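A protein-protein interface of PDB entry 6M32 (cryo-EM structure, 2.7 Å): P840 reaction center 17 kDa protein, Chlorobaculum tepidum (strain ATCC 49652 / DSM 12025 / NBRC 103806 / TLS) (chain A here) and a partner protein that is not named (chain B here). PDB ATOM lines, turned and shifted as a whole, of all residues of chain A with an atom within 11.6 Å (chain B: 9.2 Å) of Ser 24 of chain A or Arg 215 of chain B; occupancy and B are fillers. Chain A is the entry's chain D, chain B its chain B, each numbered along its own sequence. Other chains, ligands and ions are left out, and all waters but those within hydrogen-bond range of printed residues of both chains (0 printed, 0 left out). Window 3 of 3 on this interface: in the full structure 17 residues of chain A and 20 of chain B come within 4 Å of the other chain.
The backbone NH (N) of Glu 214 of chain B lies close to the backbone NH (N) of Gly 25 of chain A (3.5 Å).
The side-chain hydroxyl (OG) of Ser 24 of chain A is in hydrogen-bond range of the backbone carbonyl oxygen (O) of Gly 21 of chain A (3.2 Å). OE1 of Glu 214 of chain B lies close to O of Pro 212 of chain B (2.6 Å). NH1 of Arg 215 of chain B is in salt-bridge range of OD1 of Asp 217 of chain B, 3.5 Å away. N of Val 28 of chain A sits close to OD1 of Asn 26 of chain A, 3.4 Å away. OG of Ser 24 of chain A sits at hydrogen-bond distance from OG of Ser 20 of chain A (3.3 Å).
Glu 214 of chain B touches Ser 24 of chain A (CA to CB, 3.8 Å). Ser 24 of chain A touches Arg 215 of chain B. Gly 25 of chain A touches Thr 211 of chain B (C to CG2, 3.7 Å). Gly 25 of chain A touches Pro 212 of chain B (O to CD, 3.2 Å). N of Asn 26 of chain A touches CG2 of Thr 211 of chain B, 3.8 Å away.
Gly 21 of chain A touches none of the printed residues of chain B. Of chain B, only Thr 211, Pro 212 and Glu 214 come within 4 Å of Gly 25 of chain A. Printed residues of chain B within 4 Å of Asn 26 of chain A: Thr 211. Of the printed residues of chain A, Thr 211 of chain B touches Gly 25 (3.7 Å) and Asn 26 (3.8 Å). Pro 212 of chain B touches just one residue of chain A: Gly 25. Pro 213 of chain B touches none of the printed residues of chain A. Of chain A, only Ser 24 comes within 4 Å of Arg 215 of chain B. The nearest printed residue of chain A that does not touch Arg 215 of chain B is Gly 25 of chain A (5.0 Å). The nearest printed residue of chain B that does not touch Asn 26 of chain A is Pro 212 of chain B (5.0 Å).
Of the 8 printed residues of chain B, 4 touch a printed residue of chain A. Printed residues of chain B that touch a printed residue of chain A: Thr 211, Pro 212, Glu 214 and Arg 215. Hydrophobic or aromatic side chains of chain B that line the printed part of chain A: Pro 212. Of the 18 printed residues of chain A, 3 touch a printed residue of chain B. Among the printed residues, 6 pairs touch across the chains.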
ATOM      1  N   SER A  20      14.288  -3.914 -13.223  1.00  0.00           N
ATOM      2  CA  SER A  20      14.077  -2.524 -13.613  1.00  0.00           C
ATOM      3  C   SER A  20      14.284  -1.584 -12.430  1.00  0.00           C
ATOM      4  O   SER A  20      14.816  -1.983 -11.393  1.00  0.00           O
ATOM      5  CB  SER A  20      12.675  -2.337 -14.196  1.00  0.00           C
ATOM      6  OG  SER A  20      11.680  -2.773 -13.286  1.00  0.00           O
ATOM      7  N   GLY A  21      13.859  -0.333 -12.594  1.00  0.00           N
ATOM      8  CA  GLY A  21      14.037   0.679 -11.581  1.00  0.00           C
ATOM      9  C   GLY A  21      13.297   0.362 -10.298  1.00  0.00           C
ATOM     10  O   GLY A  21      12.240  -0.276 -10.302  1.00  0.00           O
ATOM     11  N   PRO A  22      13.856   0.797  -9.165  1.00  0.00           N
ATOM     12  CA  PRO A  22      13.198   0.542  -7.875  1.00  0.00           C
ATOM     13  C   PRO A  22      11.844   1.205  -7.731  1.00  0.00           C
ATOM     14  O   PRO A  22      11.044   0.756  -6.902  1.00  0.00           O
ATOM     15  CB  PRO A  22      14.195   1.107  -6.853  1.00  0.00           C
ATOM     16  CG  PRO A  22      15.499   1.135  -7.565  1.00  0.00           C
ATOM     17  CD  PRO A  22      15.180   1.414  -8.998  1.00  0.00           C
ATOM     18  N   TRP A  23      11.558   2.253  -8.494  1.00  0.00           N
ATOM     19  CA  TRP A  23      10.340   3.022  -8.302  1.00  0.00           C
ATOM     20  C   TRP A  23       9.162   2.506  -9.117  1.00  0.00           C
ATOM     21  O   TRP A  23       8.050   3.021  -8.960  1.00  0.00           O
ATOM     22  CB  TRP A  23      10.598   4.494  -8.620  1.00  0.00           C
ATOM     23  CG  TRP A  23      11.838   5.030  -8.004  1.00  0.00           C
ATOM     24  CD1 TRP A  23      11.954   5.620  -6.781  1.00  0.00           C
ATOM     25  CD2 TRP A  23      13.149   5.035  -8.578  1.00  0.00           C
ATOM     26  NE1 TRP A  23      13.255   5.991  -6.556  1.00  0.00           N
ATOM     27  CE2 TRP A  23      14.009   5.642  -7.645  1.00  0.00           C
ATOM     28  CE3 TRP A  23      13.676   4.585  -9.790  1.00  0.00           C
ATOM     29  CZ2 TRP A  23      15.366   5.810  -7.887  1.00  0.00           C
ATOM     30  CZ3 TRP A  23      15.023   4.751 -10.026  1.00  0.00           C
ATOM     31  CH2 TRP A  23      15.853   5.359  -9.080  1.00  0.00           C
ATOM     32  N   SER A  24       9.364   1.496  -9.956  1.00  0.00           N
ATOM     33  CA  SER A  24       8.279   0.855 -10.686  1.00  0.00           C
ATOM     34  C   SER A  24       7.882  -0.426  -9.968  1.00  0.00           C
ATOM     35  O   SER A  24       8.737  -1.141  -9.437  1.00  0.00           O
ATOM     36  CB  SER A  24       8.681   0.538 -12.128  1.00  0.00           C
ATOM     37  OG  SER A  24       9.705  -0.439 -12.167  1.00  0.00           O
ATOM     38  N   GLY A  25       6.583  -0.712  -9.954  1.00  0.00           N
ATOM     39  CA  GLY A  25       6.106  -1.874  -9.222  1.00  0.00           C
ATOM     40  C   GLY A  25       6.282  -1.681  -7.729  1.00  0.00           C
ATOM     41  O   GLY A  25       6.018  -0.606  -7.181  1.00  0.00           O
ATOM     42  N   ASN A  26       6.738  -2.732  -7.057  1.00  0.00           N
ATOM     43  CA  ASN A  26       7.004  -2.683  -5.628  1.00  0.00           C
ATOM     44  C   ASN A  26       8.499  -2.527  -5.381  1.00  0.00           C
ATOM     45  O   ASN A  26       9.323  -3.136  -6.069  1.00  0.00           O
ATOM     46  CB  ASN A  26       6.489  -3.941  -4.929  1.00  0.00           C
ATOM     47  CG  ASN A  26       6.304  -3.739  -3.440  1.00  0.00           C
ATOM     48  OD1 ASN A  26       6.774  -2.753  -2.875  1.00  0.00           O
ATOM     49  ND2 ASN A  26       5.615  -4.674  -2.796  1.00  0.00           N
ATOM     50  N   ALA A  27       8.839  -1.703  -4.393  1.00  0.00           N
ATOM     51  CA  ALA A  27      10.233  -1.446  -4.062  1.00  0.00           C
ATOM     52  C   ALA A  27      10.885  -2.589  -3.297  1.00  0.00           C
ATOM     53  O   ALA A  27      12.117  -2.673  -3.278  1.00  0.00           O
ATOM     54  CB  ALA A  27      10.343  -0.156  -3.250  1.00  0.00           C
ATOM     55  N   VAL A  28      10.097  -3.460  -2.666  1.00  0.00           N
ATOM     56  CA  VAL A  28      10.667  -4.570  -1.914  1.00  0.00           C
ATOM     57  C   VAL A  28      11.349  -5.562  -2.848  1.00  0.00           C
ATOM     58  O   VAL A  28      12.456  -6.037  -2.571  1.00  0.00           O
ATOM     59  CB  VAL A  28       9.577  -5.251  -1.065  1.00  0.00           C
ATOM     60  CG1 VAL A  28       8.503  -5.853  -1.953  1.00  0.00           C
ATOM     61  CG2 VAL A  28      10.189  -6.320  -0.185  1.00  0.00           C
ATOM     62  N   HIS A  29      10.716  -5.872  -3.972  1.00  0.00           N
ATOM     63  CA  HIS A  29      11.134  -6.993  -4.796  1.00  0.00           C
ATOM     64  C   HIS A  29      11.976  -6.530  -5.978  1.00  0.00           C
ATOM     65  O   HIS A  29      11.833  -5.415  -6.482  1.00  0.00           O
ATOM     66  CB  HIS A  29       9.912  -7.758  -5.292  1.00  0.00           C
ATOM     67  CG  HIS A  29       9.038  -8.255  -4.187  1.00  0.00           C
ATOM     68  ND1 HIS A  29       7.663  -8.182  -4.238  1.00  0.00           N
ATOM     69  CD2 HIS A  29       9.340  -8.851  -3.010  1.00  0.00           C
ATOM     70  CE1 HIS A  29       7.156  -8.704  -3.138  1.00  0.00           C
ATOM     71  NE2 HIS A  29       8.151  -9.114  -2.373  1.00  0.00           N
ATOM     72  N   LYS A  30      12.869  -7.416  -6.414  1.00  0.00           N
ATOM     73  CA  LYS A  30      13.698  -7.169  -7.584  1.00  0.00           C
ATOM     74  C   LYS A  30      12.999  -7.522  -8.888  1.00  0.00           C
ATOM     75  O   LYS A  30      13.505  -7.166  -9.958  1.00  0.00           O
ATOM     76  CB  LYS A  30      15.008  -7.957  -7.476  1.00  0.00           C
ATOM     77  CG  LYS A  30      15.567  -8.031  -6.063  1.00  0.00           C
ATOM     78  CD  LYS A  30      15.917  -6.648  -5.532  1.00  0.00           C
ATOM     79  CE  LYS A  30      16.955  -5.960  -6.405  1.00  0.00           C
ATOM     80  NZ  LYS A  30      18.271  -6.649  -6.345  1.00  0.00           N
ATOM     81  N   ALA A  31      11.860  -8.206  -8.826  1.00  0.00           N
ATOM     82  CA  ALA A  31      11.074  -8.523 -10.010  1.00  0.00           C
ATOM     83  C   ALA A  31       9.668  -8.907  -9.570  1.00  0.00           C
ATOM     84  O   ALA A  31       9.387  -9.060  -8.379  1.00  0.00           O
ATOM     85  CB  ALA A  31      11.717  -9.639 -10.835  1.00  0.00           C
ATOM     86  N   GLU A  32       8.788  -9.061 -10.555  1.00  0.00           N
ATOM     87  CA  GLU A  32       7.388  -9.354 -10.284  1.00  0.00           C
ATOM     88  C   GLU A  32       7.244 -10.707  -9.596  1.00  0.00           C
ATOM     89  O   GLU A  32       7.723 -11.726 -10.098  1.00  0.00           O
ATOM     90  CB  GLU A  32       6.602  -9.332 -11.594  1.00  0.00           C
ATOM     91  CG  GLU A  32       5.111  -9.576 -11.465  1.00  0.00           C
ATOM     92  CD  GLU A  32       4.394  -8.483 -10.699  1.00  0.00           C
ATOM     93  OE1 GLU A  32       4.892  -7.338 -10.683  1.00  0.00           O
ATOM     94  OE2 GLU A  32       3.323  -8.768 -10.122  1.00  0.00           O
ATOM     95  N   LYS A  33       6.565 -10.715  -8.453  1.00  0.00           N
ATOM     96  CA  LYS A  33       6.389 -11.911  -7.642  1.00  0.00           C
ATOM     97  C   LYS A  33       5.021 -12.533  -7.890  1.00  0.00           C
ATOM     98  O   LYS A  33       4.030 -11.831  -8.101  1.00  0.00           O
ATOM     99  CB  LYS A  33       6.547 -11.587  -6.154  1.00  0.00           C
ATOM    100  CG  LYS A  33       6.331 -12.779  -5.234  1.00  0.00           C
ATOM    101  CD  LYS A  33       6.430 -12.400  -3.770  1.00  0.00           C
ATOM    102  CE  LYS A  33       7.874 -12.294  -3.330  1.00  0.00           C
ATOM    103  NZ  LYS A  33       7.980 -12.136  -1.857  1.00  0.00           N
ATOM    104  N   ALA A  54       1.563 -10.301  -6.956  1.00  0.00           N
ATOM    105  CA  ALA A  54       1.559  -9.692  -5.631  1.00  0.00           C
ATOM    106  C   ALA A  54       0.377  -8.745  -5.462  1.00  0.00           C
ATOM    107  O   ALA A  54      -0.259  -8.722  -4.403  1.00  0.00           O
ATOM    108  CB  ALA A  54       2.876  -8.958  -5.387  1.00  0.00           C
ATOM    109  N   SER A  55       0.071  -7.957  -6.494  1.00  0.00           N
ATOM    110  CA  SER A  55      -1.058  -7.039  -6.444  1.00  0.00           C
ATOM    111  C   SER A  55      -2.405  -7.750  -6.484  1.00  0.00           C
ATOM    112  O   SER A  55      -3.406  -7.172  -6.053  1.00  0.00           O
ATOM    113  CB  SER A  55      -0.976  -6.040  -7.597  1.00  0.00           C
ATOM    114  OG  SER A  55      -2.115  -5.199  -7.620  1.00  0.00           O
ATOM    115  N   ARG A  58      -5.231 -10.834 -11.152  1.00  0.00           N
ATOM    116  CA  ARG A  58      -5.309 -11.812 -12.224  1.00  0.00           C
ATOM    117  C   ARG A  58      -5.204 -13.208 -11.629  1.00  0.00           C
ATOM    118  O   ARG A  58      -4.824 -13.386 -10.470  1.00  0.00           O
ATOM    119  CB  ARG A  58      -4.204 -11.596 -13.263  1.00  0.00           C
ATOM    120  CG  ARG A  58      -4.140 -10.207 -13.863  1.00  0.00           C
ATOM    121  CD  ARG A  58      -2.704  -9.814 -14.155  1.00  0.00           C
ATOM    122  NE  ARG A  58      -2.619  -8.569 -14.910  1.00  0.00           N
ATOM    123  CZ  ARG A  58      -2.710  -7.362 -14.367  1.00  0.00           C
ATOM    124  NH1 ARG A  58      -2.885  -7.233 -13.060  1.00  0.00           N
ATOM    125  NH2 ARG A  58      -2.622  -6.281 -15.129  1.00  0.00           N
ATOM    126  N   GLU A  74      12.787 -12.908 -14.671  1.00  0.00           N
ATOM    127  CA  GLU A  74      11.782 -11.890 -14.388  1.00  0.00           C
ATOM    128  C   GLU A  74      10.640 -12.365 -13.498  1.00  0.00           C
ATOM    129  O   GLU A  74      10.011 -11.537 -12.831  1.00  0.00           O
ATOM    130  CB  GLU A  74      11.244 -11.336 -15.718  1.00  0.00           C
ATOM    131  CG  GLU A  74      10.355 -10.097 -15.631  1.00  0.00           C
ATOM    132  CD  GLU A  74       8.909 -10.414 -15.338  1.00  0.00           C
ATOM    133  OE1 GLU A  74       8.462 -11.510 -15.724  1.00  0.00           O
ATOM    134  OE2 GLU A  74       8.220  -9.573 -14.723  1.00  0.00           O
ATOM    135  N   THR B 211      -0.134  -1.027  -5.055  1.00  0.00           N
ATOM    136  CA  THR B 211       1.163  -1.078  -5.707  1.00  0.00           C
ATOM    137  C   THR B 211       1.218  -0.103  -6.876  1.00  0.00           C
ATOM    138  O   THR B 211       0.256   0.002  -7.644  1.00  0.00           O
ATOM    139  CB  THR B 211       1.454  -2.501  -6.205  1.00  0.00           C
ATOM    140  OG1 THR B 211       1.042  -3.445  -5.210  1.00  0.00           O
ATOM    141  CG2 THR B 211       2.937  -2.683  -6.475  1.00  0.00           C
ATOM    142  N   PRO B 212       2.326   0.617  -7.037  1.00  0.00           N
ATOM    143  CA  PRO B 212       2.490   1.509  -8.196  1.00  0.00           C
ATOM    144  C   PRO B 212       2.401   0.737  -9.501  1.00  0.00           C
ATOM    145  O   PRO B 212       2.535  -0.493  -9.507  1.00  0.00           O
ATOM    146  CB  PRO B 212       3.894   2.092  -7.982  1.00  0.00           C
ATOM    147  CG  PRO B 212       4.060   2.083  -6.505  1.00  0.00           C
ATOM    148  CD  PRO B 212       3.371   0.834  -6.024  1.00  0.00           C
ATOM    149  N   PRO B 213       2.176   1.426 -10.638  1.00  0.00           N
ATOM    150  CA  PRO B 213       1.765   0.724 -11.867  1.00  0.00           C
ATOM    151  C   PRO B 213       2.867   0.148 -12.757  1.00  0.00           C
ATOM    152  O   PRO B 213       2.596  -0.149 -13.924  1.00  0.00           O
ATOM    153  CB  PRO B 213       0.974   1.804 -12.616  1.00  0.00           C
ATOM    154  CG  PRO B 213       1.590   3.082 -12.182  1.00  0.00           C
ATOM    155  CD  PRO B 213       2.047   2.890 -10.766  1.00  0.00           C
ATOM    156  N   GLU B 214       4.089  -0.020 -12.240  1.00  0.00           N
ATOM    157  CA  GLU B 214       5.220  -0.674 -12.926  1.00  0.00           C
ATOM    158  C   GLU B 214       5.353  -0.236 -14.390  1.00  0.00           C
ATOM    159  O   GLU B 214       5.106  -0.990 -15.332  1.00  0.00           O
ATOM    160  CB  GLU B 214       5.236  -2.213 -12.825  1.00  0.00           C
ATOM    161  CG  GLU B 214       4.037  -3.057 -13.255  1.00  0.00           C
ATOM    162  CD  GLU B 214       2.859  -2.956 -12.314  1.00  0.00           C
ATOM    163  OE1 GLU B 214       2.994  -2.294 -11.272  1.00  0.00           O
ATOM    164  OE2 GLU B 214       1.809  -3.565 -12.596  1.00  0.00           O
ATOM    165  N   ARG B 215       5.754   1.015 -14.549  1.00  0.00           N
ATOM    166  CA  ARG B 215       6.253   1.515 -15.818  1.00  0.00           C
ATOM    167  C   ARG B 215       7.672   0.998 -16.073  1.00  0.00           C
ATOM    168  O   ARG B 215       8.182   0.133 -15.358  1.00  0.00           O
ATOM    169  CB  ARG B 215       6.209   3.034 -15.805  1.00  0.00           C
ATOM    170  CG  ARG B 215       4.968   3.603 -15.148  1.00  0.00           C
ATOM    171  CD  ARG B 215       5.142   5.084 -15.052  1.00  0.00           C
ATOM    172  NE  ARG B 215       5.009   5.693 -16.364  1.00  0.00           N
ATOM    173  CZ  ARG B 215       6.039   6.203 -17.032  1.00  0.00           C
ATOM    174  NH1 ARG B 215       7.256   6.156 -16.509  1.00  0.00           N
ATOM    175  NH2 ARG B 215       5.855   6.747 -18.225  1.00  0.00           N
ATOM    176  N   LEU B 216       8.325   1.531 -17.111  1.00  0.00           N
ATOM    177  CA  LEU B 216       9.718   1.214 -17.413  1.00  0.00           C
ATOM    178  C   LEU B 216      10.360   2.414 -18.102  1.00  0.00           C
ATOM    179  O   LEU B 216       9.671   3.210 -18.738  1.00  0.00           O
ATOM    180  CB  LEU B 216       9.827  -0.068 -18.265  1.00  0.00           C
ATOM    181  CG  LEU B 216       9.313  -0.187 -19.702  1.00  0.00           C
ATOM    182  CD1 LEU B 216      10.384   0.221 -20.682  1.00  0.00           C
ATOM    183  CD2 LEU B 216       8.865  -1.598 -19.997  1.00  0.00           C
ATOM    184  N   ASP B 217      11.688   2.529 -17.992  1.00  0.00           N
ATOM    185  CA  ASP B 217      12.353   3.829 -17.985  1.00  0.00           C
ATOM    186  C   ASP B 217      13.577   3.849 -18.905  1.00  0.00           C
ATOM    187  O   ASP B 217      14.075   2.797 -19.317  1.00  0.00           O
ATOM    188  CB  ASP B 217      12.743   4.157 -16.522  1.00  0.00           C
ATOM    189  CG  ASP B 217      11.564   4.482 -15.647  1.00  0.00           C
ATOM    190  OD1 ASP B 217      10.468   4.740 -16.188  1.00  0.00           O
ATOM    191  OD2 ASP B 217      11.752   4.544 -14.417  1.00  0.00           O
ATOM    192  N   PHE B 218      14.049   5.062 -19.237  1.00  0.00           N
ATOM    193  CA  PHE B 218      15.329   5.270 -19.917  1.00  0.00           C
ATOM    194  C   PHE B 218      15.947   6.594 -19.476  1.00  0.00           C
ATOM    195  O   PHE B 218      15.579   7.172 -18.452  1.00  0.00           O
ATOM    196  CB  PHE B 218      15.219   5.278 -21.451  1.00  0.00           C
ATOM    197  CG  PHE B 218      14.235   6.280 -22.008  1.00  0.00           C
ATOM    198  CD1 PHE B 218      13.094   5.850 -22.620  1.00  0.00           C
ATOM    199  CD2 PHE B 218      14.477   7.642 -21.970  1.00  0.00           C
ATOM    200  CE1 PHE B 218      12.182   6.742 -23.154  1.00  0.00           C
ATOM    201  CE2 PHE B 218      13.570   8.541 -22.500  1.00  0.00           C
ATOM    202  CZ  PHE B 218      12.420   8.084 -23.095  1.00  0.00           C
